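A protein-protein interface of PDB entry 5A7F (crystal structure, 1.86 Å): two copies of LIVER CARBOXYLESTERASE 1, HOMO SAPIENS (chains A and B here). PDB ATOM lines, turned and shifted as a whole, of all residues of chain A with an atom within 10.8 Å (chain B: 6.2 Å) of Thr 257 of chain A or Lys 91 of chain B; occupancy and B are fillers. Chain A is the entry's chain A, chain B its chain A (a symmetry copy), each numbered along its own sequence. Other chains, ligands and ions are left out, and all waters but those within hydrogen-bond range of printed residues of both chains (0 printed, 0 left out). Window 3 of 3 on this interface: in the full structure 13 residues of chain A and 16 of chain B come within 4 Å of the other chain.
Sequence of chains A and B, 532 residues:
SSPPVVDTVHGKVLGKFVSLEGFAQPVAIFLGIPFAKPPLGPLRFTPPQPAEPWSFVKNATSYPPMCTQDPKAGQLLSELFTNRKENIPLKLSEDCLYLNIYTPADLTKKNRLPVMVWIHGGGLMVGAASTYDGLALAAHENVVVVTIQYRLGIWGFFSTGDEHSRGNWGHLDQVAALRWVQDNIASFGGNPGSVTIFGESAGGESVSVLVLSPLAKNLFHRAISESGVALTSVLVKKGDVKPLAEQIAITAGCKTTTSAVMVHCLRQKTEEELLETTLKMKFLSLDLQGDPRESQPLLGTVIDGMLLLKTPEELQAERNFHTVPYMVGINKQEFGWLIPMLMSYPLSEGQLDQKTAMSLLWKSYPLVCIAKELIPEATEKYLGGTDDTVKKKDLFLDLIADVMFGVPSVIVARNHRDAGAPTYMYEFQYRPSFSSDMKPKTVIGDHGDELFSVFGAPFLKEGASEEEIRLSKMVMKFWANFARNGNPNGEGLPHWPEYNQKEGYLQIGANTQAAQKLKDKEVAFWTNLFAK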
ATOM      1  N   PHE A 158      26.052   7.263 -31.733  1.00  0.00           N
ATOM      2  CA  PHE A 158      26.131   5.910 -31.237  1.00  0.00           C
ATOM      3  C   PHE A 158      27.557   5.364 -31.240  1.00  0.00           C
ATOM      4  O   PHE A 158      28.191   5.308 -32.282  1.00  0.00           O
ATOM      5  CB  PHE A 158      25.263   4.964 -32.027  1.00  0.00           C
ATOM      6  CG  PHE A 158      25.292   3.583 -31.477  1.00  0.00           C
ATOM      7  CD1 PHE A 158      24.560   3.273 -30.331  1.00  0.00           C
ATOM      8  CD2 PHE A 158      26.054   2.606 -32.078  1.00  0.00           C
ATOM      9  CE1 PHE A 158      24.616   1.999 -29.801  1.00  0.00           C
ATOM     10  CE2 PHE A 158      26.106   1.320 -31.548  1.00  0.00           C
ATOM     11  CZ  PHE A 158      25.358   1.007 -30.421  1.00  0.00           C
ATOM     12  N   THR A 160      30.074   2.182 -29.492  1.00  0.00           N
ATOM     13  CA  THR A 160      30.309   0.973 -28.711  1.00  0.00           C
ATOM     14  C   THR A 160      31.615   1.057 -27.907  1.00  0.00           C
ATOM     15  O   THR A 160      31.955   0.118 -27.205  1.00  0.00           O
ATOM     16  CB  THR A 160      30.402  -0.274 -29.615  1.00  0.00           C
ATOM     17  OG1 THR A 160      31.355  -0.065 -30.690  1.00  0.00           O
ATOM     18  CG2 THR A 160      29.069  -0.634 -30.171  1.00  0.00           C
ATOM     19  N   ASP A 162      34.491   0.996 -29.214  1.00  0.00           N
ATOM     20  CA  ASP A 162      35.566   0.286 -29.942  1.00  0.00           C
ATOM     21  C   ASP A 162      35.376   0.474 -31.444  1.00  0.00           C
ATOM     22  O   ASP A 162      34.538   1.290 -31.877  1.00  0.00           O
ATOM     23  CB  ASP A 162      35.568  -1.189 -29.538  1.00  0.00           C
ATOM     24  CG  ASP A 162      34.249  -1.891 -29.884  1.00  0.00           C
ATOM     25  OD1 ASP A 162      33.584  -1.528 -30.906  1.00  0.00           O
ATOM     26  OD2 ASP A 162      33.868  -2.820 -29.130  1.00  0.00           O
ATOM     27  N   HIS A 164      34.102  -1.105 -33.871  1.00  0.00           N
ATOM     28  CA  HIS A 164      32.872  -1.438 -34.572  1.00  0.00           C
ATOM     29  C   HIS A 164      31.882  -0.282 -34.639  1.00  0.00           C
ATOM     30  O   HIS A 164      31.032  -0.313 -35.520  1.00  0.00           O
ATOM     31  CB  HIS A 164      32.189  -2.631 -33.949  1.00  0.00           C
ATOM     32  CG  HIS A 164      33.062  -3.832 -33.883  1.00  0.00           C
ATOM     33  ND1 HIS A 164      33.493  -4.494 -35.011  1.00  0.00           N
ATOM     34  CD2 HIS A 164      33.660  -4.439 -32.835  1.00  0.00           C
ATOM     35  CE1 HIS A 164      34.305  -5.475 -34.651  1.00  0.00           C
ATOM     36  NE2 HIS A 164      34.409  -5.469 -33.341  1.00  0.00           N
ATOM     37  N   LYS A 242      30.005   1.695 -23.120  1.00  0.00           N
ATOM     38  CA  LYS A 242      29.341   0.439 -23.446  1.00  0.00           C
ATOM     39  C   LYS A 242      27.969   0.206 -22.731  1.00  0.00           C
ATOM     40  O   LYS A 242      27.057  -0.303 -23.363  1.00  0.00           O
ATOM     41  CB  LYS A 242      30.314  -0.727 -23.202  1.00  0.00           C
ATOM     42  CG  LYS A 242      29.955  -2.023 -23.900  1.00  0.00           C
ATOM     43  CD  LYS A 242      30.548  -2.050 -25.301  1.00  0.00           C
ATOM     44  CE  LYS A 242      30.054  -3.241 -26.098  1.00  0.00           C
ATOM     45  NZ  LYS A 242      30.769  -4.518 -25.835  1.00  0.00           N
ATOM     46  N   ALA A 245      25.428   2.318 -24.680  1.00  0.00           N
ATOM     47  CA  ALA A 245      25.245   1.603 -25.937  1.00  0.00           C
ATOM     48  C   ALA A 245      24.341   0.377 -25.795  1.00  0.00           C
ATOM     49  O   ALA A 245      23.454   0.180 -26.610  1.00  0.00           O
ATOM     50  CB  ALA A 245      26.568   1.207 -26.524  1.00  0.00           C
ATOM     51  N   GLU A 246      24.541  -0.424 -24.744  1.00  0.00           N
ATOM     52  CA  GLU A 246      23.716  -1.589 -24.513  1.00  0.00           C
ATOM     53  C   GLU A 246      22.265  -1.250 -24.217  1.00  0.00           C
ATOM     54  O   GLU A 246      21.351  -1.940 -24.657  1.00  0.00           O
ATOM     55  CB  GLU A 246      24.294  -2.439 -23.384  1.00  0.00           C
ATOM     56  CG  GLU A 246      25.570  -3.130 -23.826  1.00  0.00           C
ATOM     57  CD  GLU A 246      26.299  -3.840 -22.699  1.00  0.00           C
ATOM     58  OE1 GLU A 246      25.704  -4.003 -21.624  1.00  0.00           O
ATOM     59  OE2 GLU A 246      27.467  -4.236 -22.898  1.00  0.00           O
ATOM     60  N   GLN A 247      22.057  -0.193 -23.446  1.00  0.00           N
ATOM     61  CA  GLN A 247      20.705   0.243 -23.135  1.00  0.00           C
ATOM     62  C   GLN A 247      19.963   0.645 -24.402  1.00  0.00           C
ATOM     63  O   GLN A 247      18.819   0.288 -24.582  1.00  0.00           O
ATOM     64  CB  GLN A 247      20.764   1.404 -22.168  1.00  0.00           C
ATOM     65  CG  GLN A 247      19.394   1.895 -21.769  1.00  0.00           C
ATOM     66  CD  GLN A 247      19.431   2.832 -20.588  1.00  0.00           C
ATOM     67  OE1 GLN A 247      20.482   3.423 -20.266  1.00  0.00           O
ATOM     68  NE2 GLN A 247      18.278   2.996 -19.936  1.00  0.00           N
ATOM     69  N   ALA A 249      20.671  -0.443 -27.493  1.00  0.00           N
ATOM     70  CA  ALA A 249      20.412  -1.662 -28.274  1.00  0.00           C
ATOM     71  C   ALA A 249      19.204  -2.441 -27.758  1.00  0.00           C
ATOM     72  O   ALA A 249      18.368  -2.883 -28.557  1.00  0.00           O
ATOM     73  CB  ALA A 249      21.599  -2.545 -28.256  1.00  0.00           C
ATOM     74  N   ILE A 250      19.145  -2.584 -26.429  1.00  0.00           N
ATOM     75  CA  ILE A 250      18.073  -3.342 -25.761  1.00  0.00           C
ATOM     76  C   ILE A 250      16.720  -2.683 -26.006  1.00  0.00           C
ATOM     77  O   ILE A 250      15.729  -3.367 -26.297  1.00  0.00           O
ATOM     78  CB  ILE A 250      18.371  -3.497 -24.248  1.00  0.00           C
ATOM     79  CG1 ILE A 250      19.609  -4.398 -24.054  1.00  0.00           C
ATOM     80  CG2 ILE A 250      17.187  -4.133 -23.476  1.00  0.00           C
ATOM     81  CD1 ILE A 250      20.316  -4.150 -22.711  1.00  0.00           C
ATOM     82  N   GLY A 253      15.479  -3.410 -29.348  1.00  0.00           N
ATOM     83  CA  GLY A 253      15.164  -4.823 -29.570  1.00  0.00           C
ATOM     84  C   GLY A 253      16.342  -5.582 -30.179  1.00  0.00           C
ATOM     85  O   GLY A 253      16.159  -6.569 -30.884  1.00  0.00           O
ATOM     86  N   CYS A 254      17.561  -5.113 -29.901  1.00  0.00           N
ATOM     87  CA  CYS A 254      18.781  -5.765 -30.321  1.00  0.00           C
ATOM     88  C   CYS A 254      19.461  -6.550 -29.172  1.00  0.00           C
ATOM     89  O   CYS A 254      19.507  -6.094 -28.039  1.00  0.00           O
ATOM     90  CB  CYS A 254      19.745  -4.681 -30.846  1.00  0.00           C
ATOM     91  SG  CYS A 254      19.160  -3.976 -32.394  1.00  0.00           S
ATOM     92  N   LYS A 255      20.018  -7.707 -29.498  1.00  0.00           N
ATOM     93  CA  LYS A 255      20.931  -8.442 -28.612  1.00  0.00           C
ATOM     94  C   LYS A 255      22.220  -7.668 -28.356  1.00  0.00           C
ATOM     95  O   LYS A 255      22.630  -6.832 -29.174  1.00  0.00           O
ATOM     96  CB  LYS A 255      21.348  -9.751 -29.272  1.00  0.00           C
ATOM     97  CG  LYS A 255      20.258 -10.821 -29.298  1.00  0.00           C
ATOM     98  CD  LYS A 255      20.672 -12.016 -30.153  1.00  0.00           C
ATOM     99  CE  LYS A 255      21.310 -11.526 -31.466  1.00  0.00           C
ATOM    100  NZ  LYS A 255      20.978 -12.299 -32.680  1.00  0.00           N
ATOM    101  N   THR A 256      22.858  -7.952 -27.228  1.00  0.00           N
ATOM    102  CA  THR A 256      24.028  -7.201 -26.817  1.00  0.00           C
ATOM    103  C   THR A 256      25.270  -8.111 -26.754  1.00  0.00           C
ATOM    104  O   THR A 256      26.224  -7.776 -26.090  1.00  0.00           O
ATOM    105  CB  THR A 256      23.788  -6.543 -25.444  1.00  0.00           C
ATOM    106  OG1 THR A 256      23.476  -7.556 -24.500  1.00  0.00           O
ATOM    107  CG2 THR A 256      22.621  -5.580 -25.485  1.00  0.00           C
ATOM    108  N   THR A 257      25.250  -9.231 -27.477  1.00  0.00           N
ATOM    109  CA  THR A 257      26.260 -10.273 -27.348  1.00  0.00           C
ATOM    110  C   THR A 257      27.670  -9.753 -27.566  1.00  0.00           C
ATOM    111  O   THR A 257      28.577 -10.089 -26.807  1.00  0.00           O
ATOM    112  CB  THR A 257      25.961 -11.372 -28.370  1.00  0.00           C
ATOM    113  OG1 THR A 257      24.560 -11.614 -28.321  1.00  0.00           O
ATOM    114  CG2 THR A 257      26.692 -12.667 -28.043  1.00  0.00           C
ATOM    115  N   THR A 258      27.830  -8.919 -28.592  1.00  0.00           N
ATOM    116  CA  THR A 258      29.095  -8.240 -28.916  1.00  0.00           C
ATOM    117  C   THR A 258      28.782  -6.858 -29.501  1.00  0.00           C
ATOM    118  O   THR A 258      27.631  -6.548 -29.856  1.00  0.00           O
ATOM    119  CB  THR A 258      29.926  -8.963 -29.970  1.00  0.00           C
ATOM    120  OG1 THR A 258      29.341  -8.798 -31.269  1.00  0.00           O
ATOM    121  CG2 THR A 258      30.110 -10.425 -29.649  1.00  0.00           C
ATOM    122  N   SER A 259      29.807  -6.033 -29.550  1.00  0.00           N
ATOM    123  CA  SER A 259      29.717  -4.744 -30.176  1.00  0.00           C
ATOM    124  C   SER A 259      29.225  -4.831 -31.614  1.00  0.00           C
ATOM    125  O   SER A 259      28.322  -4.086 -32.001  1.00  0.00           O
ATOM    126  CB  SER A 259      31.085  -4.040 -30.166  1.00  0.00           C
ATOM    127  OG  SER A 259      31.476  -3.656 -28.860  1.00  0.00           O
ATOM    128  N   ALA A 260      29.853  -5.707 -32.399  1.00  0.00           N
ATOM    129  CA  ALA A 260      29.544  -5.818 -33.833  1.00  0.00           C
ATOM    130  C   ALA A 260      28.100  -6.294 -34.018  1.00  0.00           C
ATOM    131  O   ALA A 260      27.397  -5.847 -34.929  1.00  0.00           O
ATOM    132  CB  ALA A 260      30.526  -6.755 -34.536  1.00  0.00           C
ATOM    133  N   VAL A 261      27.642  -7.160 -33.117  1.00  0.00           N
ATOM    134  CA  VAL A 261      26.238  -7.592 -33.148  1.00  0.00           C
ATOM    135  C   VAL A 261      25.249  -6.430 -32.925  1.00  0.00           C
ATOM    136  O   VAL A 261      24.235  -6.321 -33.613  1.00  0.00           O
ATOM    137  CB  VAL A 261      25.969  -8.750 -32.157  1.00  0.00           C
ATOM    138  CG1 VAL A 261      24.500  -8.869 -31.784  1.00  0.00           C
ATOM    139  CG2 VAL A 261      26.478 -10.045 -32.751  1.00  0.00           C
ATOM    140  N   MET A 262      25.551  -5.591 -31.957  1.00  0.00           N
ATOM    141  CA  MET A 262      24.679  -4.471 -31.620  1.00  0.00           C
ATOM    142  C   MET A 262      24.623  -3.479 -32.783  1.00  0.00           C
ATOM    143  O   MET A 262      23.560  -3.013 -33.138  1.00  0.00           O
ATOM    144  CB  MET A 262      25.197  -3.745 -30.364  1.00  0.00           C
ATOM    145  CG  MET A 262      25.131  -4.543 -29.069  1.00  0.00           C
ATOM    146  SD  MET A 262      25.569  -3.464 -27.687  1.00  0.00           S
ATOM    147  CE  MET A 262      27.326  -3.428 -27.744  1.00  0.00           C
ATOM    148  N   VAL A 263      25.777  -3.122 -33.334  1.00  0.00           N
ATOM    149  CA  VAL A 263      25.814  -2.150 -34.400  1.00  0.00           C
ATOM    150  C   VAL A 263      25.141  -2.695 -35.653  1.00  0.00           C
ATOM    151  O   VAL A 263      24.434  -1.960 -36.328  1.00  0.00           O
ATOM    152  CB  VAL A 263      27.225  -1.762 -34.858  1.00  0.00           C
ATOM    153  CG1 VAL A 263      27.078  -0.635 -35.868  1.00  0.00           C
ATOM    154  CG2 VAL A 263      28.054  -1.299 -33.691  1.00  0.00           C
ATOM    155  N   HIS A 264      25.390  -3.961 -35.969  1.00  0.00           N
ATOM    156  CA  HIS A 264      24.771  -4.591 -37.136  1.00  0.00           C
ATOM    157  C   HIS A 264      23.255  -4.646 -36.994  1.00  0.00           C
ATOM    158  O   HIS A 264      22.523  -4.269 -37.910  1.00  0.00           O
ATOM    159  CB  HIS A 264      25.355  -6.000 -37.433  1.00  0.00           C
ATOM    160  CG  HIS A 264      24.671  -6.685 -38.567  1.00  0.00           C
ATOM    161  ND1 HIS A 264      24.872  -6.311 -39.871  1.00  0.00           N
ATOM    162  CD2 HIS A 264      23.689  -7.623 -38.591  1.00  0.00           C
ATOM    163  CE1 HIS A 264      24.120  -7.055 -40.663  1.00  0.00           C
ATOM    164  NE2 HIS A 264      23.382  -7.846 -39.911  1.00  0.00           N
ATOM    165  N   CYS A 265      22.786  -5.034 -35.826  1.00  0.00           N
ATOM    166  CA  CYS A 265      21.331  -5.052 -35.560  1.00  0.00           C
ATOM    167  C   CYS A 265      20.648  -3.670 -35.691  1.00  0.00           C
ATOM    168  O   CYS A 265      19.579  -3.536 -36.319  1.00  0.00           O
ATOM    169  CB  CYS A 265      21.095  -5.646 -34.178  1.00  0.00           C
ATOM    170  SG  CYS A 265      19.342  -5.638 -33.676  1.00  0.00           S
ATOM    171  N   TYR B  63      36.207 -14.590 -22.800  1.00  0.00           N
ATOM    172  CA  TYR B  63      36.108 -15.594 -23.865  1.00  0.00           C
ATOM    173  C   TYR B  63      35.186 -15.073 -24.986  1.00  0.00           C
ATOM    174  O   TYR B  63      34.092 -14.548 -24.711  1.00  0.00           O
ATOM    175  CB  TYR B  63      35.604 -16.936 -23.343  1.00  0.00           C
ATOM    176  CG  TYR B  63      36.549 -17.591 -22.408  1.00  0.00           C
ATOM    177  CD1 TYR B  63      37.643 -18.255 -22.884  1.00  0.00           C
ATOM    178  CD2 TYR B  63      36.355 -17.520 -21.027  1.00  0.00           C
ATOM    179  CE1 TYR B  63      38.569 -18.862 -22.022  1.00  0.00           C
ATOM    180  CE2 TYR B  63      37.253 -18.137 -20.160  1.00  0.00           C
ATOM    181  CZ  TYR B  63      38.387 -18.782 -20.694  1.00  0.00           C
ATOM    182  OH  TYR B  63      39.299 -19.397 -19.892  1.00  0.00           O
ATOM    183  N   PRO B  64      35.581 -15.278 -26.247  1.00  0.00           N
ATOM    184  CA  PRO B  64      34.699 -14.893 -27.338  1.00  0.00           C
ATOM    185  C   PRO B  64      33.446 -15.788 -27.415  1.00  0.00           C
ATOM    186  O   PRO B  64      33.462 -16.891 -26.856  1.00  0.00           O
ATOM    187  CB  PRO B  64      35.538 -15.148 -28.563  1.00  0.00           C
ATOM    188  CG  PRO B  64      36.460 -16.258 -28.179  1.00  0.00           C
ATOM    189  CD  PRO B  64      36.764 -16.017 -26.724  1.00  0.00           C
ATOM    190  N   PRO B  65      32.401 -15.338 -28.130  1.00  0.00           N
ATOM    191  CA  PRO B  65      31.282 -16.288 -28.388  1.00  0.00           C
ATOM    192  C   PRO B  65      31.780 -17.458 -29.258  1.00  0.00           C
ATOM    193  O   PRO B  65      32.768 -17.331 -30.026  1.00  0.00           O
ATOM    194  CB  PRO B  65      30.232 -15.431 -29.134  1.00  0.00           C
ATOM    195  CG  PRO B  65      30.764 -14.003 -29.105  1.00  0.00           C
ATOM    196  CD  PRO B  65      32.242 -14.071 -28.882  1.00  0.00           C
ATOM    197  N   MET B  66      31.121 -18.586 -29.126  1.00  0.00           N
ATOM    198  CA  MET B  66      31.254 -19.653 -30.093  1.00  0.00           C
ATOM    199  C   MET B  66      30.363 -19.361 -31.318  1.00  0.00           C
ATOM    200  O   MET B  66      29.345 -18.647 -31.209  1.00  0.00           O
ATOM    201  CB  MET B  66      30.977 -21.029 -29.474  1.00  0.00           C
ATOM    202  CG  MET B  66      29.559 -21.308 -29.035  1.00  0.00           C
ATOM    203  SD  MET B  66      29.620 -22.877 -28.121  1.00  0.00           S
ATOM    204  CE  MET B  66      27.894 -23.156 -27.767  1.00  0.00           C
ATOM    205  N   CYS B  67      30.811 -19.823 -32.483  1.00  0.00           N
ATOM    206  CA  CYS B  67      30.059 -19.631 -33.724  1.00  0.00           C
ATOM    207  C   CYS B  67      28.679 -20.266 -33.582  1.00  0.00           C
ATOM    208  O   CYS B  67      28.463 -21.283 -32.864  1.00  0.00           O
ATOM    209  CB  CYS B  67      30.802 -20.177 -34.923  1.00  0.00           C
ATOM    210  SG  CYS B  67      32.404 -19.367 -35.251  1.00  0.00           S
ATOM    211  N   PRO B  89      30.723 -20.387 -19.166  1.00  0.00           N
ATOM    212  CA  PRO B  89      29.565 -19.998 -19.962  1.00  0.00           C
ATOM    213  C   PRO B  89      30.037 -19.487 -21.305  1.00  0.00           C
ATOM    214  O   PRO B  89      30.967 -18.679 -21.353  1.00  0.00           O
ATOM    215  CB  PRO B  89      28.941 -18.875 -19.145  1.00  0.00           C
ATOM    216  CG  PRO B  89      30.081 -18.283 -18.389  1.00  0.00           C
ATOM    217  CD  PRO B  89      30.994 -19.428 -18.079  1.00  0.00           C
ATOM    218  N   LEU B  90      29.485 -20.007 -22.390  1.00  0.00           N
ATOM    219  CA  LEU B  90      29.809 -19.458 -23.704  1.00  0.00           C
ATOM    220  C   LEU B  90      28.569 -18.918 -24.420  1.00  0.00           C
ATOM    221  O   LEU B  90      27.532 -19.541 -24.447  1.00  0.00           O
ATOM    222  CB  LEU B  90      30.576 -20.456 -24.576  1.00  0.00           C
ATOM    223  CG  LEU B  90      32.005 -20.801 -24.099  1.00  0.00           C
ATOM    224  CD1 LEU B  90      32.650 -21.846 -24.993  1.00  0.00           C
ATOM    225  CD2 LEU B  90      32.918 -19.573 -24.015  1.00  0.00           C
ATOM    226  N   LYS B  91      28.707 -17.716 -24.953  1.00  0.00           N
ATOM    227  CA  LYS B  91      27.687 -17.114 -25.811  1.00  0.00           C
ATOM    228  C   LYS B  91      27.785 -17.733 -27.215  1.00  0.00           C
ATOM    229  O   LYS B  91      28.847 -18.239 -27.594  1.00  0.00           O
ATOM    230  CB  LYS B  91      27.921 -15.612 -25.933  1.00  0.00           C
ATOM    231  CG  LYS B  91      28.090 -14.874 -24.618  1.00  0.00           C
ATOM    232  CD  LYS B  91      26.849 -14.987 -23.769  1.00  0.00           C
ATOM    233  CE  LYS B  91      26.826 -13.937 -22.667  1.00  0.00           C
ATOM    234  NZ  LYS B  91      25.413 -13.601 -22.322  1.00  0.00           N
ATOM    235  N   LEU B  92      26.673 -17.691 -27.946  1.00  0.00           N
ATOM    236  CA  LEU B  92      26.573 -18.017 -29.376  1.00  0.00           C
ATOM    237  C   LEU B  92      26.486 -16.731 -30.180  1.00  0.00           C
ATOM    238  O   LEU B  92      25.684 -15.871 -29.834  1.00  0.00           O
ATOM    239  CB  LEU B  92      25.237 -18.731 -29.664  1.00  0.00           C
ATOM    240  CG  LEU B  92      24.921 -20.147 -29.208  1.00  0.00           C
ATOM    241  CD1 LEU B  92      23.642 -20.614 -29.875  1.00  0.00           C
ATOM    242  CD2 LEU B  92      26.038 -21.100 -29.559  1.00  0.00           C
ATOM    243  N   SER B  93      27.234 -16.628 -31.272  1.00  0.00           N
ATOM    244  CA  SER B  93      27.102 -15.518 -32.196  1.00  0.00           C
ATOM    245  C   SER B  93      27.669 -15.842 -33.548  1.00  0.00           C
ATOM    246  O   SER B  93      28.614 -16.650 -33.655  1.00  0.00           O
ATOM    247  CB  SER B  93      27.839 -14.301 -31.626  1.00  0.00           C
ATOM    248  OG  SER B  93      27.591 -13.129 -32.376  1.00  0.00           O
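The side-chain hydroxyl (OG1) of Thr 258 of chain A lies close to the backbone NH (N) of Ala 260 of chain A, at 3.3 Å. The side-chain sulfur (SG) of Cys 254 of chain A is disulfide-bonded to the side-chain sulfur (SG) of Cys 265 of chain A (2.1 Å). The backbone NH (N) of Val 261 of chain A lies within hydrogen-bond range of the side-chain hydroxyl (OG1) of Thr 258 of chain A, at 3.0 Å. The backbone carbonyl oxygen (O) of Met 66 of chain B sits at hydrogen-bond distance from the backbone NH (N) of Ser 93 of chain B (2.9 Å). The backbone NH (N) of Met 66 of chain B sits at hydrogen-bond distance from the backbone carbonyl oxygen (O) of Lys 91 of chain B (2.8 Å).
Lys 91 of chain B touches Thr 257 of chain A (CB to CG2, 3.8 Å). Leu 92 of chain B touches Thr 257 of chain A (O to CG2, 3.8 Å). Pro 65 of chain B touches Thr 258 of chain A (CG to CG2, 3.7 Å). Val 261 of chain A touches Ser 93 of chain B (CG2 to OG, 3.3 Å).
Of chain B, only Lys 91 (3.8 Å) and Leu 92 (3.8 Å) come within 4 Å of Thr 257 of chain A. Of chain A, only Thr 258 comes within 4 Å of Pro 65 of chain B. No residue of chain A comes within 4 Å of Met 66 of chain B. No residue of chain A comes within 4 Å of Leu 90 of chain B. Leu 92 of chain B touches just one residue of chain A: Thr 257. Of the printed residues of chain A, Ser 93 of chain B touches Val 261. Of the printed residues of chain B, Thr 258 of chain A touches Pro 65 (3.7 Å). Of the printed residues of chain B, Val 261 of chain A touches Ser 93 (3.3 Å).
Of the 23 printed residues of chain A, 3 touch a printed residue of chain B. Hydrophobic or aromatic side chains of chain A within 4 Å of the printed part of chain B: Val 261. Along chain A the printed residues that touch a printed residue of chain B span positions 257 to 261. Of the 10 printed residues of chain B, 4 touch a printed residue of chain A. Along chain B the printed residues that touch a printed residue of chain A span positions 65 to 93. Among the printed residues, no Asp or Glu carboxylate lies within 4 Å of a Lys or Arg side-chain nitrogen of the other chain.
No position is printed for both chains. Of the 4 pairs that touch across the chains among the printed residues, none has its exchanged pair printed and touching as well.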
